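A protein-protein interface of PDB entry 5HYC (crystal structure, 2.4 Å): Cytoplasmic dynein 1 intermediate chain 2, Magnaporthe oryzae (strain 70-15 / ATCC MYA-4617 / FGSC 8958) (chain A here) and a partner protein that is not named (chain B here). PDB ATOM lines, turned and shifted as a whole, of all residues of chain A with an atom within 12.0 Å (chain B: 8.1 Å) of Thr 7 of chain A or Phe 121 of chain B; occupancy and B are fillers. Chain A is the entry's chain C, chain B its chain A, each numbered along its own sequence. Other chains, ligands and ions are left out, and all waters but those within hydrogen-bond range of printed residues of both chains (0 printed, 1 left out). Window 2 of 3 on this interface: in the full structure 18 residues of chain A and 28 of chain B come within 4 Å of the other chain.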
ATOM      1  N   LEU A   6       6.661  -4.660 -20.615  1.00  0.00           N
ATOM      2  CA  LEU A   6       7.097  -3.273 -20.760  1.00  0.00           C
ATOM      3  C   LEU A   6       7.440  -2.653 -19.409  1.00  0.00           C
ATOM      4  O   LEU A   6       8.614  -2.494 -19.082  1.00  0.00           O
ATOM      5  CB  LEU A   6       6.023  -2.442 -21.464  1.00  0.00           C
ATOM      6  CG  LEU A   6       6.477  -1.070 -21.959  1.00  0.00           C
ATOM      7  CD1 LEU A   6       7.785  -1.193 -22.721  1.00  0.00           C
ATOM      8  CD2 LEU A   6       5.404  -0.429 -22.827  1.00  0.00           C
ATOM      9  N   THR A   7       6.419  -2.305 -18.629  1.00  0.00           N
ATOM     10  CA  THR A   7       6.631  -1.729 -17.302  1.00  0.00           C
ATOM     11  C   THR A   7       6.264  -2.720 -16.187  1.00  0.00           C
ATOM     12  O   THR A   7       5.180  -3.299 -16.196  1.00  0.00           O
ATOM     13  CB  THR A   7       5.822  -0.424 -17.115  1.00  0.00           C
ATOM     14  OG1 THR A   7       4.424  -0.709 -17.182  1.00  0.00           O
ATOM     15  CG2 THR A   7       6.179   0.591 -18.185  1.00  0.00           C
ATOM     16  N   THR A   8       7.173  -2.908 -15.229  1.00  0.00           N
ATOM     17  CA  THR A   8       6.995  -3.910 -14.177  1.00  0.00           C
ATOM     18  C   THR A   8       7.173  -3.367 -12.753  1.00  0.00           C
ATOM     19  O   THR A   8       7.378  -2.173 -12.550  1.00  0.00           O
ATOM     20  CB  THR A   8       7.979  -5.072 -14.366  1.00  0.00           C
ATOM     21  OG1 THR A   8       9.314  -4.605 -14.146  1.00  0.00           O
ATOM     22  CG2 THR A   8       7.868  -5.647 -15.775  1.00  0.00           C
ATOM     23  N   VAL A   9       7.097  -4.260 -11.770  1.00  0.00           N
ATOM     24  CA  VAL A   9       7.254  -3.890 -10.364  1.00  0.00           C
ATOM     25  C   VAL A   9       8.593  -4.397  -9.831  1.00  0.00           C
ATOM     26  O   VAL A   9       8.721  -5.576  -9.518  1.00  0.00           O
ATOM     27  CB  VAL A   9       6.104  -4.465  -9.489  1.00  0.00           C
ATOM     28  CG1 VAL A   9       6.262  -4.050  -8.052  1.00  0.00           C
ATOM     29  CG2 VAL A   9       4.768  -4.007  -9.985  1.00  0.00           C
ATOM     30  N   PRO A  10       9.608  -3.518  -9.751  1.00  0.00           N
ATOM     31  CA  PRO A  10      10.916  -3.950  -9.246  1.00  0.00           C
ATOM     32  C   PRO A  10      11.113  -3.873  -7.736  1.00  0.00           C
ATOM     33  O   PRO A  10      10.268  -3.382  -6.988  1.00  0.00           O
ATOM     34  CB  PRO A  10      11.883  -2.984  -9.939  1.00  0.00           C
ATOM     35  CG  PRO A  10      11.105  -1.761 -10.110  1.00  0.00           C
ATOM     36  CD  PRO A  10       9.726  -2.243 -10.479  1.00  0.00           C
ATOM     37  N   LEU A  11      12.275  -4.361  -7.322  1.00  0.00           N
ATOM     38  CA  LEU A  11      12.697  -4.392  -5.931  1.00  0.00           C
ATOM     39  C   LEU A  11      12.671  -3.016  -5.260  1.00  0.00           C
ATOM     40  O   LEU A  11      12.716  -1.991  -5.930  1.00  0.00           O
ATOM     41  CB  LEU A  11      14.105  -4.985  -5.840  1.00  0.00           C
ATOM     42  CG  LEU A  11      14.399  -6.357  -6.466  1.00  0.00           C
ATOM     43  CD1 LEU A  11      14.497  -6.320  -7.994  1.00  0.00           C
ATOM     44  CD2 LEU A  11      15.660  -6.977  -5.857  1.00  0.00           C
ATOM     45  N   THR A  12      12.623  -2.997  -3.931  1.00  0.00           N
ATOM     46  CA  THR A  12      12.531  -1.746  -3.179  1.00  0.00           C
ATOM     47  C   THR A  12      13.912  -1.305  -2.669  1.00  0.00           C
ATOM     48  O   THR A  12      14.763  -2.153  -2.432  1.00  0.00           O
ATOM     49  CB  THR A  12      11.541  -1.892  -2.006  1.00  0.00           C
ATOM     50  OG1 THR A  12      11.881  -3.044  -1.251  1.00  0.00           O
ATOM     51  CG2 THR A  12      10.128  -2.094  -2.516  1.00  0.00           C
ATOM     52  N   THR A  13      14.141   0.009  -2.541  1.00  0.00           N
ATOM     53  CA  THR A  13      15.429   0.561  -2.070  1.00  0.00           C
ATOM     54  C   THR A  13      15.261   1.499  -0.856  1.00  0.00           C
ATOM     55  O   THR A  13      14.142   1.734  -0.443  1.00  0.00           O
ATOM     56  CB  THR A  13      16.151   1.333  -3.187  1.00  0.00           C
ATOM     57  OG1 THR A  13      15.764   2.709  -3.143  1.00  0.00           O
ATOM     58  CG2 THR A  13      15.806   0.759  -4.546  1.00  0.00           C
ATOM     59  N   THR B 118      11.611   3.232  -1.242  1.00  0.00           N
ATOM     60  CA  THR B 118      10.835   3.543  -2.432  1.00  0.00           C
ATOM     61  C   THR B 118      10.577   2.313  -3.292  1.00  0.00           C
ATOM     62  O   THR B 118      11.484   1.538  -3.572  1.00  0.00           O
ATOM     63  CB  THR B 118      11.533   4.625  -3.296  1.00  0.00           C
ATOM     64  OG1 THR B 118      11.692   5.819  -2.528  1.00  0.00           O
ATOM     65  CG2 THR B 118      10.695   4.961  -4.512  1.00  0.00           C
ATOM     66  N   GLY B 119       9.325   2.143  -3.701  1.00  0.00           N
ATOM     67  CA  GLY B 119       8.967   1.157  -4.703  1.00  0.00           C
ATOM     68  C   GLY B 119       8.457   1.819  -5.974  1.00  0.00           C
ATOM     69  O   GLY B 119       8.032   2.974  -5.956  1.00  0.00           O
ATOM     70  N   ALA B 120       8.492   1.089  -7.082  1.00  0.00           N
ATOM     71  CA  ALA B 120       8.123   1.668  -8.367  1.00  0.00           C
ATOM     72  C   ALA B 120       7.455   0.683  -9.319  1.00  0.00           C
ATOM     73  O   ALA B 120       7.709  -0.508  -9.278  1.00  0.00           O
ATOM     74  CB  ALA B 120       9.359   2.274  -9.032  1.00  0.00           C
ATOM     75  N   PHE B 121       6.574   1.204 -10.163  1.00  0.00           N
ATOM     76  CA  PHE B 121       6.008   0.452 -11.279  1.00  0.00           C
ATOM     77  C   PHE B 121       6.498   1.154 -12.536  1.00  0.00           C
ATOM     78  O   PHE B 121       5.950   2.170 -12.953  1.00  0.00           O
ATOM     79  CB  PHE B 121       4.486   0.397 -11.203  1.00  0.00           C
ATOM     80  CG  PHE B 121       3.852  -0.414 -12.300  1.00  0.00           C
ATOM     81  CD1 PHE B 121       4.093  -1.773 -12.399  1.00  0.00           C
ATOM     82  CD2 PHE B 121       3.007   0.181 -13.219  1.00  0.00           C
ATOM     83  CE1 PHE B 121       3.515  -2.524 -13.395  1.00  0.00           C
ATOM     84  CE2 PHE B 121       2.429  -0.561 -14.222  1.00  0.00           C
ATOM     85  CZ  PHE B 121       2.682  -1.919 -14.312  1.00  0.00           C
ATOM     86  N   TRP B 122       7.548   0.581 -13.116  1.00  0.00           N
ATOM     87  CA  TRP B 122       8.511   1.297 -13.947  1.00  0.00           C
ATOM     88  C   TRP B 122       8.947   0.494 -15.128  1.00  0.00           C
ATOM     89  O   TRP B 122       8.706  -0.692 -15.179  1.00  0.00           O
ATOM     90  CB  TRP B 122       9.787   1.580 -13.161  1.00  0.00           C
ATOM     91  CG  TRP B 122       9.908   2.862 -12.527  1.00  0.00           C
ATOM     92  CD1 TRP B 122       9.014   3.880 -12.542  1.00  0.00           C
ATOM     93  CD2 TRP B 122      11.020   3.305 -11.759  1.00  0.00           C
ATOM     94  NE1 TRP B 122       9.499   4.942 -11.810  1.00  0.00           N
ATOM     95  CE2 TRP B 122      10.734   4.611 -11.323  1.00  0.00           C
ATOM     96  CE3 TRP B 122      12.228   2.721 -11.387  1.00  0.00           C
ATOM     97  CZ2 TRP B 122      11.615   5.342 -10.541  1.00  0.00           C
ATOM     98  CZ3 TRP B 122      13.096   3.446 -10.612  1.00  0.00           C
ATOM     99  CH2 TRP B 122      12.790   4.743 -10.201  1.00  0.00           C
ATOM    100  N   ASN B 123       9.685   1.134 -16.022  1.00  0.00           N
ATOM    101  CA  ASN B 123      10.543   0.421 -16.948  1.00  0.00           C
ATOM    102  C   ASN B 123      11.870   0.166 -16.233  1.00  0.00           C
ATOM    103  O   ASN B 123      12.628   1.089 -15.962  1.00  0.00           O
ATOM    104  CB  ASN B 123      10.746   1.214 -18.237  1.00  0.00           C
ATOM    105  CG  ASN B 123      11.322   0.372 -19.366  1.00  0.00           C
ATOM    106  OD1 ASN B 123      12.180  -0.482 -19.156  1.00  0.00           O
ATOM    107  ND2 ASN B 123      10.849   0.623 -20.578  1.00  0.00           N
ATOM    108  N   ASP B 124      12.128  -1.098 -15.918  1.00  0.00           N
ATOM    109  CA  ASP B 124      13.269  -1.502 -15.099  1.00  0.00           C
ATOM    110  C   ASP B 124      14.617  -1.195 -15.757  1.00  0.00           C
ATOM    111  O   ASP B 124      15.610  -0.959 -15.072  1.00  0.00           O
ATOM    112  CB  ASP B 124      13.158  -2.996 -14.788  1.00  0.00           C
ATOM    113  CG  ASP B 124      14.305  -3.513 -13.932  1.00  0.00           C
ATOM    114  OD1 ASP B 124      14.795  -2.753 -13.072  1.00  0.00           O
ATOM    115  OD2 ASP B 124      14.701  -4.690 -14.106  1.00  0.00           O
ATOM    116  N   LYS B 125      14.648  -1.176 -17.082  1.00  0.00           N
ATOM    117  CA  LYS B 125      15.907  -0.979 -17.795  1.00  0.00           C
ATOM    118  C   LYS B 125      16.249   0.483 -18.092  1.00  0.00           C
ATOM    119  O   LYS B 125      17.393   0.796 -18.407  1.00  0.00           O
ATOM    120  CB  LYS B 125      15.892  -1.783 -19.100  1.00  0.00           C
ATOM    121  CG  LYS B 125      15.925  -3.287 -18.882  1.00  0.00           C
ATOM    122  CD  LYS B 125      14.911  -4.023 -19.726  1.00  0.00           C
ATOM    123  CE  LYS B 125      15.162  -5.535 -19.705  1.00  0.00           C
ATOM    124  NZ  LYS B 125      15.632  -6.053 -18.385  1.00  0.00           N
ATOM    125  N   THR B 126      15.275   1.376 -17.972  1.00  0.00           N
ATOM    126  CA  THR B 126      15.512   2.777 -18.294  1.00  0.00           C
ATOM    127  C   THR B 126      15.369   3.709 -17.097  1.00  0.00           C
ATOM    128  O   THR B 126      16.010   4.749 -17.037  1.00  0.00           O
ATOM    129  CB  THR B 126      14.561   3.261 -19.394  1.00  0.00           C
ATOM    130  OG1 THR B 126      13.208   3.122 -18.949  1.00  0.00           O
ATOM    131  CG2 THR B 126      14.756   2.453 -20.638  1.00  0.00           C
ATOM    132  N   ASP B 127      14.528   3.324 -16.150  1.00  0.00           N
ATOM    133  CA  ASP B 127      14.178   4.196 -15.041  1.00  0.00           C
ATOM    134  C   ASP B 127      14.922   3.822 -13.769  1.00  0.00           C
ATOM    135  O   ASP B 127      15.323   2.671 -13.586  1.00  0.00           O
ATOM    136  CB  ASP B 127      12.664   4.170 -14.839  1.00  0.00           C
ATOM    137  CG  ASP B 127      11.913   4.444 -16.135  1.00  0.00           C
ATOM    138  OD1 ASP B 127      12.494   5.113 -17.007  1.00  0.00           O
ATOM    139  OD2 ASP B 127      10.760   4.002 -16.291  1.00  0.00           O
ATOM    140  N   ILE B 151      12.987   9.206 -15.114  1.00  0.00           N
ATOM    141  CA  ILE B 151      12.103   8.403 -15.921  1.00  0.00           C
ATOM    142  C   ILE B 151      12.420   8.690 -17.378  1.00  0.00           C
ATOM    143  O   ILE B 151      12.324   9.829 -17.828  1.00  0.00           O
ATOM    144  CB  ILE B 151      10.633   8.709 -15.642  1.00  0.00           C
ATOM    145  CG1 ILE B 151      10.370   8.837 -14.138  1.00  0.00           C
ATOM    146  CG2 ILE B 151       9.749   7.657 -16.284  1.00  0.00           C
ATOM    147  CD1 ILE B 151       9.768   7.604 -13.507  1.00  0.00           C
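Of the 8 printed residues of chain A, 7 touch a printed residue of chain B. Along chain A the printed residues that touch a printed residue of chain B span positions 6 to 13. Among the printed residues, no Asp or Glu carboxylate lies within 4 Å of a Lys or Arg side-chain nitrogen of the other chain.
The backbone carbonyl oxygen (O) of Thr 13 of chain A lies within hydrogen-bond range of the backbone NH (N) of Thr 118 of chain B, at 3.0 Å. The backbone NH (N) of Thr 8 of chain A lies within hydrogen-bond range of the backbone carbonyl oxygen (O) of Trp 122 of chain B (2.7 Å).
The backbone NH (N) of Lys 125 of chain B lies close to the side-chain amide oxygen (OD1) of Asn 123 of chain B (3.3 Å). The backbone NH of Asn 123 of chain B lies within hydrogen-bond range of the side-chain carboxylate of Asp 127 of chain B, 3.1 Å away.
Leu 6 of chain A touches Asn 123 of chain B. Phe 121 of chain B touches Thr 7 of chain A. Trp 122 of chain B touches Thr 7 of chain A. O of Thr 8 of chain A touches O of Ala 120 of chain B, 3.7 Å away. Thr 8 of chain A touches Phe 121 of chain B (O to CA, 3.2 Å). Val 9 of chain A touches Ala 120 of chain B. Val 9 of chain A touches Phe 121 of chain B (CG2 to CD1, 3.4 Å). Ala 120 of chain B touches Pro 10 of chain A (O to CD, 2.9 Å). Thr 118 of chain B touches Thr 12 of chain A.
Of chain B, only Phe 121 (3.3 Å) and Trp 122 (3.1 Å) come within 4 Å of Thr 7 of chain A. Of chain A, only Thr 7 (3.3 Å), Thr 8 (3.2 Å) and Val 9 (3.4 Å) come within 4 Å of Phe 121 of chain B. No residue of chain A comes within 4 Å of Gly 119 of chain B. Asn 123 of chain B touches just one residue of chain A: Leu 6 (3.95 Å). Printed residues of chain B within 4 Å of Thr 8 of chain A: Ala 120 (3.7 Å), Phe 121 (3.2 Å) and Trp 122 (2.7 Å). Printed residues of chain B within 4 Å of Pro 10 of chain A: Ala 120. Of the printed residues of chain B, Leu 6 of chain A touches Asn 123. Of the printed residues of chain B, Thr 12 of chain A touches Thr 118. The nearest residue of chain B that does not touch Thr 7 of chain A is Asn 123 of chain B (4.2 Å). The nearest residue of chain A that does not touch Phe 121 of chain B is Pro 10 of chain A (4.7 Å). The nearest printed residue of chain B that does not touch Thr 13 of chain A is Gly 119 of chain B (5.4 Å).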
